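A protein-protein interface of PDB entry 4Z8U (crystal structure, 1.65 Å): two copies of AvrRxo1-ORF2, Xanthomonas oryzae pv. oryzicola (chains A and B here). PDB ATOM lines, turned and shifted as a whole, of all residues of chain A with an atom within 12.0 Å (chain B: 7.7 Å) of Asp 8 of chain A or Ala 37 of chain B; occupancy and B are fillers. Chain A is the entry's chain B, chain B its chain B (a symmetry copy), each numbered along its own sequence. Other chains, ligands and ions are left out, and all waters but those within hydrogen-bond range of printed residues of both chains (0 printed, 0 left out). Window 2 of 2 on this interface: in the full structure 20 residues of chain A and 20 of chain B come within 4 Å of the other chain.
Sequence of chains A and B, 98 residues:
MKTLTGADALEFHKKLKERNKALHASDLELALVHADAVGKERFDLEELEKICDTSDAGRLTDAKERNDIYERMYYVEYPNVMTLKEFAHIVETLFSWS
No position is printed for both chains.
Of the 9 pairs that touch across the chains among the printed residues, none has its exchanged pair printed and touching as well.
CE of Met 1 of chain A touches CD2 of His 34 of chain B, at 3.6 Å.
Val 38 of chain B touches Lys 2 of chain A.
Leu 4 of chain A touches Ala 37 of chain B.
Asp 8 of chain A touches Val 33 of chain B.
Asp 8 of chain A touches Ala 37 of chain B.
Val 33 of chain B touches Glu 11 of chain A.
Val 33 of chain B touches Phe 12 of chain A (CG1 to N, 3.98 Å).
A ring nitrogen (NE2) of His 34 of chain B is in hydrogen-bond range of the side-chain amino group of Lys 2 of chain A (3.4 Å).
OD1 of Asp 8 of chain A sits close to OD1 of Asp 36 of chain B.
Ala 37 of chain B touches just these residues of chain A: Leu 4 and Asp 8.
No residue of chain B comes within 4 Å of Ala 7 of chain A.
His 34 of chain B touches just these residues of chain A: Met 1 and Lys 2.
No residue of chain A comes within 4 Å of Ala 35 of chain B.
Of chain A, only Asp 8 comes within 4 Å of Asp 36 of chain B.
Gly 39 of chain B touches none of the printed residues of chain A.
Of the printed residues of chain A, Val 33 of chain B touches Asp 8, Glu 11 and Phe 12.
Of the printed residues of chain B, Glu 11 of chain A touches Val 33 (3.8 Å).
Of the printed residues of chain B, Phe 12 of chain A touches Val 33 (3.98 Å).
Of the printed residues of chain B, Lys 2 of chain A touches His 34 (3.4 Å) and Val 38 (3.1 Å).
The nearest residue of chain B that does not touch Asp 8 of chain A is Val 38 of chain B (5.9 Å).
The nearest residue of chain A that does not touch Ala 37 of chain B is Lys 2 of chain A (5.3 Å).
The nearest printed residue of chain B that does not touch Met 1 of chain A is Val 38 of chain B (6.2 Å).
Of the 11 printed residues of chain B, 5 touch a printed residue of chain A.
Printed residues of chain B that touch a printed residue of chain A: Val 33, His 34, Asp 36, Ala 37 and Val 38.
Hydrophobic or aromatic side chains of chain B within 4 Å of the printed part of chain A: Val 33, His 34, Ala 37 and Val 38.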
ATOM      1  N   MET A   1     -10.948 -10.636  -9.386  1.00  0.00           N
ATOM      2  CA  MET A   1     -12.192 -10.055  -8.806  1.00  0.00           C
ATOM      3  C   MET A   1     -13.434 -10.782  -9.376  1.00  0.00           C
ATOM      4  O   MET A   1     -13.381 -11.410 -10.414  1.00  0.00           O
ATOM      5  CB  MET A   1     -12.151  -8.512  -9.006  1.00  0.00           C
ATOM      6  CG  MET A   1     -12.293  -7.978 -10.473  1.00  0.00           C
ATOM      7  SD  MET A   1     -12.128  -6.019 -10.346  1.00  0.00           S
ATOM      8  CE  MET A   1     -13.920  -5.634  -9.767  1.00  0.00           C
ATOM      9  N   LYS A   2     -14.552 -10.659  -8.655  1.00  0.00           N
ATOM     10  CA  LYS A   2     -15.822 -11.163  -9.061  1.00  0.00           C
ATOM     11  C   LYS A   2     -16.235 -10.628 -10.473  1.00  0.00           C
ATOM     12  O   LYS A   2     -16.140  -9.394 -10.719  1.00  0.00           O
ATOM     13  CB  LYS A   2     -16.842 -10.746  -7.986  1.00  0.00           C
ATOM     14  CG  LYS A   2     -16.539  -9.381  -7.280  1.00  0.00           C
ATOM     15  CD  LYS A   2     -15.762  -9.455  -5.924  1.00  0.00           C
ATOM     16  CE  LYS A   2     -14.271  -9.024  -5.943  1.00  0.00           C
ATOM     17  NZ  LYS A   2     -14.086  -7.534  -6.001  1.00  0.00           N
ATOM     18  N   THR A   3     -16.679 -11.545 -11.347  1.00  0.00           N
ATOM     19  CA  THR A   3     -17.202 -11.156 -12.694  1.00  0.00           C
ATOM     20  C   THR A   3     -18.526 -10.445 -12.621  1.00  0.00           C
ATOM     21  O   THR A   3     -19.414 -10.920 -11.988  1.00  0.00           O
ATOM     22  CB  THR A   3     -17.346 -12.410 -13.676  1.00  0.00           C
ATOM     23  OG1 THR A   3     -16.039 -12.970 -13.829  1.00  0.00           O
ATOM     24  CG2 THR A   3     -17.830 -11.999 -14.975  1.00  0.00           C
ATOM     25  N   LEU A   4     -18.623  -9.293 -13.257  1.00  0.00           N
ATOM     26  CA  LEU A   4     -19.931  -8.660 -13.441  1.00  0.00           C
ATOM     27  C   LEU A   4     -20.688  -9.364 -14.564  1.00  0.00           C
ATOM     28  O   LEU A   4     -20.196  -9.508 -15.689  1.00  0.00           O
ATOM     29  CB  LEU A   4     -19.828  -7.171 -13.768  1.00  0.00           C
ATOM     30  CG  LEU A   4     -18.908  -6.313 -12.909  1.00  0.00           C
ATOM     31  CD1 LEU A   4     -18.973  -4.871 -13.392  1.00  0.00           C
ATOM     32  CD2 LEU A   4     -19.231  -6.467 -11.441  1.00  0.00           C
ATOM     33  N   THR A   5     -21.966  -9.658 -14.317  1.00  0.00           N
ATOM     34  CA  THR A   5     -22.716 -10.450 -15.256  1.00  0.00           C
ATOM     35  C   THR A   5     -24.089  -9.777 -15.470  1.00  0.00           C
ATOM     36  O   THR A   5     -24.455  -8.867 -14.692  1.00  0.00           O
ATOM     37  CB  THR A   5     -23.031 -11.876 -14.742  1.00  0.00           C
ATOM     38  OG1 THR A   5     -23.918 -11.736 -13.623  1.00  0.00           O
ATOM     39  CG2 THR A   5     -21.752 -12.546 -14.236  1.00  0.00           C
ATOM     40  N   GLY A   6     -24.807 -10.192 -16.504  1.00  0.00           N
ATOM     41  CA  GLY A   6     -26.131  -9.728 -16.731  1.00  0.00           C
ATOM     42  C   GLY A   6     -26.319  -8.239 -16.647  1.00  0.00           C
ATOM     43  O   GLY A   6     -25.642  -7.461 -17.340  1.00  0.00           O
ATOM     44  N   ALA A   7     -27.319  -7.823 -15.863  1.00  0.00           N
ATOM     45  CA  ALA A   7     -27.649  -6.365 -15.879  1.00  0.00           C
ATOM     46  C   ALA A   7     -26.515  -5.547 -15.254  1.00  0.00           C
ATOM     47  O   ALA A   7     -26.332  -4.392 -15.659  1.00  0.00           O
ATOM     48  CB  ALA A   7     -28.995  -6.103 -15.136  1.00  0.00           C
ATOM     49  N   ASP A   8     -25.817  -6.095 -14.274  1.00  0.00           N
ATOM     50  CA  ASP A   8     -24.680  -5.309 -13.659  1.00  0.00           C
ATOM     51  C   ASP A   8     -23.617  -5.070 -14.720  1.00  0.00           C
ATOM     52  O   ASP A   8     -23.029  -3.961 -14.804  1.00  0.00           O
ATOM     53  CB  ASP A   8     -24.070  -6.066 -12.509  1.00  0.00           C
ATOM     54  CG  ASP A   8     -24.951  -6.054 -11.259  1.00  0.00           C
ATOM     55  OD1 ASP A   8     -25.852  -5.191 -11.132  1.00  0.00           O
ATOM     56  OD2 ASP A   8     -24.718  -6.932 -10.421  1.00  0.00           O
ATOM     57  N   ALA A   9     -23.353  -6.066 -15.545  1.00  0.00           N
ATOM     58  CA  ALA A   9     -22.341  -5.846 -16.583  1.00  0.00           C
ATOM     59  C   ALA A   9     -22.775  -4.796 -17.571  1.00  0.00           C
ATOM     60  O   ALA A   9     -22.005  -3.896 -17.944  1.00  0.00           O
ATOM     61  CB  ALA A   9     -21.979  -7.170 -17.319  1.00  0.00           C
ATOM     62  N   LEU A  10     -24.065  -4.881 -17.993  1.00  0.00           N
ATOM     63  CA  LEU A  10     -24.522  -3.945 -18.945  1.00  0.00           C
ATOM     64  C   LEU A  10     -24.513  -2.492 -18.368  1.00  0.00           C
ATOM     65  O   LEU A  10     -24.166  -1.552 -19.069  1.00  0.00           O
ATOM     66  CB  LEU A  10     -25.944  -4.263 -19.396  1.00  0.00           C
ATOM     67  CG  LEU A  10     -26.045  -5.355 -20.487  1.00  0.00           C
ATOM     68  CD1 LEU A  10     -27.534  -5.732 -20.676  1.00  0.00           C
ATOM     69  CD2 LEU A  10     -25.497  -4.848 -21.820  1.00  0.00           C
ATOM     70  N   GLU A  11     -24.977  -2.390 -17.129  1.00  0.00           N
ATOM     71  CA  GLU A  11     -24.976  -1.004 -16.479  1.00  0.00           C
ATOM     72  C   GLU A  11     -23.541  -0.472 -16.266  1.00  0.00           C
ATOM     73  O   GLU A  11     -23.304   0.683 -16.556  1.00  0.00           O
ATOM     74  CB  GLU A  11     -25.756  -1.024 -15.198  1.00  0.00           C
ATOM     75  CG  GLU A  11     -25.961   0.372 -14.596  1.00  0.00           C
ATOM     76  CD  GLU A  11     -26.925   1.241 -15.394  1.00  0.00           C
ATOM     77  OE1 GLU A  11     -27.483   0.774 -16.414  1.00  0.00           O
ATOM     78  OE2 GLU A  11     -27.138   2.424 -14.992  1.00  0.00           O
ATOM     79  N   PHE A  12     -22.601  -1.326 -15.871  1.00  0.00           N
ATOM     80  CA  PHE A  12     -21.194  -0.879 -15.802  1.00  0.00           C
ATOM     81  C   PHE A  12     -20.730  -0.349 -17.171  1.00  0.00           C
ATOM     82  O   PHE A  12     -20.121   0.717 -17.291  1.00  0.00           O
ATOM     83  CB  PHE A  12     -20.288  -2.028 -15.314  1.00  0.00           C
ATOM     84  CG  PHE A  12     -18.915  -1.585 -14.818  1.00  0.00           C
ATOM     85  CD1 PHE A  12     -18.726  -1.224 -13.502  1.00  0.00           C
ATOM     86  CD2 PHE A  12     -17.868  -1.449 -15.695  1.00  0.00           C
ATOM     87  CE1 PHE A  12     -17.493  -0.800 -13.017  1.00  0.00           C
ATOM     88  CE2 PHE A  12     -16.586  -1.054 -15.198  1.00  0.00           C
ATOM     89  CZ  PHE A  12     -16.420  -0.776 -13.848  1.00  0.00           C
ATOM     90  N   HIS A  13     -20.983  -1.117 -18.234  1.00  0.00           N
ATOM     91  CA  HIS A  13     -20.537  -0.742 -19.568  1.00  0.00           C
ATOM     92  C   HIS A  13     -21.191   0.573 -19.997  1.00  0.00           C
ATOM     93  O   HIS A  13     -20.554   1.479 -20.486  1.00  0.00           O
ATOM     94  CB  HIS A  13     -20.913  -1.937 -20.497  1.00  0.00           C
ATOM     95  CG  HIS A  13     -20.639  -1.690 -21.952  1.00  0.00           C
ATOM     96  ND1 HIS A  13     -19.396  -1.938 -22.516  1.00  0.00           N
ATOM     97  CD2 HIS A  13     -21.430  -1.210 -22.961  1.00  0.00           C
ATOM     98  CE1 HIS A  13     -19.455  -1.691 -23.820  1.00  0.00           C
ATOM     99  NE2 HIS A  13     -20.717  -1.204 -24.107  1.00  0.00           N
ATOM    100  N   LYS A  14     -22.499   0.733 -19.675  1.00  0.00           N
ATOM    101  CA  LYS A  14     -23.216   1.957 -20.089  1.00  0.00           C
ATOM    102  C   LYS A  14     -22.623   3.220 -19.345  1.00  0.00           C
ATOM    103  O   LYS A  14     -22.336   4.251 -19.993  1.00  0.00           O
ATOM    104  CB  LYS A  14     -24.712   1.863 -19.590  1.00  0.00           C
ATOM    105  CG  LYS A  14     -25.482   3.060 -20.094  1.00  0.00           C
ATOM    106  CD  LYS A  14     -26.972   2.785 -19.723  1.00  0.00           C
ATOM    107  CE  LYS A  14     -27.831   3.881 -20.312  1.00  0.00           C
ATOM    108  NZ  LYS A  14     -29.244   3.601 -19.805  1.00  0.00           N
ATOM    109  N   LYS A  15     -22.449   3.097 -18.062  1.00  0.00           N
ATOM    110  CA  LYS A  15     -21.842   4.194 -17.256  1.00  0.00           C
ATOM    111  C   LYS A  15     -20.380   4.509 -17.669  1.00  0.00           C
ATOM    112  O   LYS A  15     -19.949   5.696 -17.729  1.00  0.00           O
ATOM    113  CB  LYS A  15     -21.988   3.906 -15.744  1.00  0.00           C
ATOM    114  CG  LYS A  15     -23.466   3.928 -15.285  1.00  0.00           C
ATOM    115  CD  LYS A  15     -24.128   5.307 -15.606  1.00  0.00           C
ATOM    116  CE  LYS A  15     -25.509   5.416 -14.925  1.00  0.00           C
ATOM    117  NZ  LYS A  15     -26.146   6.701 -15.460  1.00  0.00           N
ATOM    118  N   LEU A  16     -19.608   3.461 -17.961  1.00  0.00           N
ATOM    119  CA  LEU A  16     -18.244   3.642 -18.393  1.00  0.00           C
ATOM    120  C   LEU A  16     -18.189   4.362 -19.750  1.00  0.00           C
ATOM    121  O   LEU A  16     -17.321   5.195 -20.015  1.00  0.00           O
ATOM    122  CB  LEU A  16     -17.511   2.270 -18.443  1.00  0.00           C
ATOM    123  CG  LEU A  16     -16.043   2.330 -18.836  1.00  0.00           C
ATOM    124  CD1 LEU A  16     -15.165   3.241 -17.957  1.00  0.00           C
ATOM    125  CD2 LEU A  16     -15.539   0.886 -18.779  1.00  0.00           C
ATOM    126  N   LYS A  17     -19.091   4.017 -20.692  1.00  0.00           N
ATOM    127  CA  LYS A  17     -19.188   4.720 -21.936  1.00  0.00           C
ATOM    128  C   LYS A  17     -19.421   6.226 -21.727  1.00  0.00           C
ATOM    129  O   LYS A  17     -18.786   7.047 -22.390  1.00  0.00           O
ATOM    130  CB  LYS A  17     -20.315   4.124 -22.778  1.00  0.00           C
ATOM    131  CG  LYS A  17     -19.953   2.920 -23.617  1.00  0.00           C
ATOM    132  CD  LYS A  17     -21.239   2.322 -24.311  1.00  0.00           C
ATOM    133  CE  LYS A  17     -21.768   3.365 -25.303  1.00  0.00           C
ATOM    134  NZ  LYS A  17     -22.770   2.637 -26.161  1.00  0.00           N
ATOM    135  N   ALA B  31     -19.013   2.760  -8.833  1.00  0.00           N
ATOM    136  CA  ALA B  31     -18.874   2.141  -7.553  1.00  0.00           C
ATOM    137  C   ALA B  31     -20.192   1.458  -7.079  1.00  0.00           C
ATOM    138  O   ALA B  31     -20.122   0.374  -6.499  1.00  0.00           O
ATOM    139  CB  ALA B  31     -18.395   3.127  -6.513  1.00  0.00           C
ATOM    140  N   LEU B  32     -21.291   2.112  -7.358  1.00  0.00           N
ATOM    141  CA  LEU B  32     -22.600   1.551  -6.970  1.00  0.00           C
ATOM    142  C   LEU B  32     -22.883   0.275  -7.760  1.00  0.00           C
ATOM    143  O   LEU B  32     -23.425  -0.664  -7.181  1.00  0.00           O
ATOM    144  CB  LEU B  32     -23.707   2.548  -7.257  1.00  0.00           C
ATOM    145  CG  LEU B  32     -23.818   3.726  -6.196  1.00  0.00           C
ATOM    146  CD1 LEU B  32     -24.847   4.731  -6.750  1.00  0.00           C
ATOM    147  CD2 LEU B  32     -24.212   3.228  -4.829  1.00  0.00           C
ATOM    148  N   VAL B  33     -22.554   0.249  -9.055  1.00  0.00           N
ATOM    149  CA  VAL B  33     -22.663  -1.056  -9.791  1.00  0.00           C
ATOM    150  C   VAL B  33     -21.866  -2.136  -9.161  1.00  0.00           C
ATOM    151  O   VAL B  33     -22.378  -3.225  -8.908  1.00  0.00           O
ATOM    152  CB  VAL B  33     -22.350  -0.899 -11.272  1.00  0.00           C
ATOM    153  CG1 VAL B  33     -22.496  -2.257 -12.000  1.00  0.00           C
ATOM    154  CG2 VAL B  33     -23.275   0.099 -11.884  1.00  0.00           C
ATOM    155  N   HIS B  34     -20.551  -1.894  -8.982  1.00  0.00           N
ATOM    156  CA  HIS B  34     -19.712  -2.828  -8.310  1.00  0.00           C
ATOM    157  C   HIS B  34     -20.232  -3.296  -6.954  1.00  0.00           C
ATOM    158  O   HIS B  34     -20.192  -4.513  -6.615  1.00  0.00           O
ATOM    159  CB  HIS B  34     -18.275  -2.281  -8.206  1.00  0.00           C
ATOM    160  CG  HIS B  34     -17.332  -3.155  -7.356  1.00  0.00           C
ATOM    161  ND1 HIS B  34     -17.157  -2.956  -6.029  1.00  0.00           N
ATOM    162  CD2 HIS B  34     -16.558  -4.266  -7.695  1.00  0.00           C
ATOM    163  CE1 HIS B  34     -16.280  -3.872  -5.525  1.00  0.00           C
ATOM    164  NE2 HIS B  34     -15.921  -4.683  -6.550  1.00  0.00           N
ATOM    165  N   ALA B  35     -20.722  -2.348  -6.138  1.00  0.00           N
ATOM    166  CA  ALA B  35     -21.204  -2.671  -4.801  1.00  0.00           C
ATOM    167  C   ALA B  35     -22.442  -3.623  -4.844  1.00  0.00           C
ATOM    168  O   ALA B  35     -22.487  -4.598  -4.097  1.00  0.00           O
ATOM    169  CB  ALA B  35     -21.552  -1.423  -4.010  1.00  0.00           C
ATOM    170  N   ASP B  36     -23.340  -3.332  -5.750  1.00  0.00           N
ATOM    171  CA  ASP B  36     -24.450  -4.245  -6.015  1.00  0.00           C
ATOM    172  C   ASP B  36     -23.986  -5.651  -6.365  1.00  0.00           C
ATOM    173  O   ASP B  36     -24.495  -6.639  -5.796  1.00  0.00           O
ATOM    174  CB  ASP B  36     -25.371  -3.672  -7.108  1.00  0.00           C
ATOM    175  CG  ASP B  36     -26.530  -4.612  -7.466  1.00  0.00           C
ATOM    176  OD1 ASP B  36     -26.309  -5.541  -8.265  1.00  0.00           O
ATOM    177  OD2 ASP B  36     -27.653  -4.405  -6.953  1.00  0.00           O
ATOM    178  N   ALA B  37     -23.046  -5.778  -7.297  1.00  0.00           N
ATOM    179  CA  ALA B  37     -22.506  -7.050  -7.732  1.00  0.00           C
ATOM    180  C   ALA B  37     -21.834  -7.890  -6.630  1.00  0.00           C
ATOM    181  O   ALA B  37     -21.817  -9.144  -6.701  1.00  0.00           O
ATOM    182  CB  ALA B  37     -21.491  -6.811  -8.860  1.00  0.00           C
ATOM    183  N   VAL B  38     -21.240  -7.248  -5.621  1.00  0.00           N
ATOM    184  CA  VAL B  38     -20.460  -7.987  -4.666  1.00  0.00           C
ATOM    185  C   VAL B  38     -21.358  -8.088  -3.372  1.00  0.00           C
ATOM    186  O   VAL B  38     -20.997  -8.683  -2.425  1.00  0.00           O
ATOM    187  CB  VAL B  38     -19.046  -7.418  -4.399  1.00  0.00           C
ATOM    188  CG1 VAL B  38     -18.280  -7.284  -5.717  1.00  0.00           C
ATOM    189  CG2 VAL B  38     -19.149  -6.058  -3.725  1.00  0.00           C
ATOM    190  N   GLY B  39     -22.535  -7.499  -3.389  1.00  0.00           N
ATOM    191  CA  GLY B  39     -23.421  -7.591  -2.232  1.00  0.00           C
ATOM    192  C   GLY B  39     -22.957  -6.764  -1.054  1.00  0.00           C
ATOM    193  O   GLY B  39     -23.169  -7.136   0.121  1.00  0.00           O
ATOM    194  N   LYS B  40     -22.334  -5.607  -1.352  1.00  0.00           N
ATOM    195  CA  LYS B  40     -21.952  -4.701  -0.271  1.00  0.00           C
ATOM    196  C   LYS B  40     -23.226  -4.204   0.375  1.00  0.00           C
ATOM    197  O   LYS B  40     -24.220  -3.832  -0.311  1.00  0.00           O
ATOM    198  CB  LYS B  40     -21.109  -3.548  -0.912  1.00  0.00           C
ATOM    199  CG  LYS B  40     -20.769  -2.353  -0.007  1.00  0.00           C
ATOM    200  CD  LYS B  40     -19.684  -1.541  -0.722  1.00  0.00           C
ATOM    201  CE  LYS B  40     -19.377  -0.303   0.130  1.00  0.00           C
ATOM    202  NZ  LYS B  40     -17.905  -0.104   0.082  1.00  0.00           N
ATOM    203  N   MET B  82     -17.300  -4.006   3.173  1.00  0.00           N
ATOM    204  CA  MET B  82     -18.596  -4.617   2.834  1.00  0.00           C
ATOM    205  C   MET B  82     -19.771  -4.203   3.710  1.00  0.00           C
ATOM    206  O   MET B  82     -20.925  -4.333   3.333  1.00  0.00           O
ATOM    207  CB  MET B  82     -18.387  -6.152   2.842  1.00  0.00           C
ATOM    208  CG  MET B  82     -17.503  -6.741   1.733  1.00  0.00           C
ATOM    209  SD  MET B  82     -18.305  -6.333  -0.024  1.00  0.00           S
ATOM    210  CE  MET B  82     -17.020  -4.918  -0.526  1.00  0.00           C
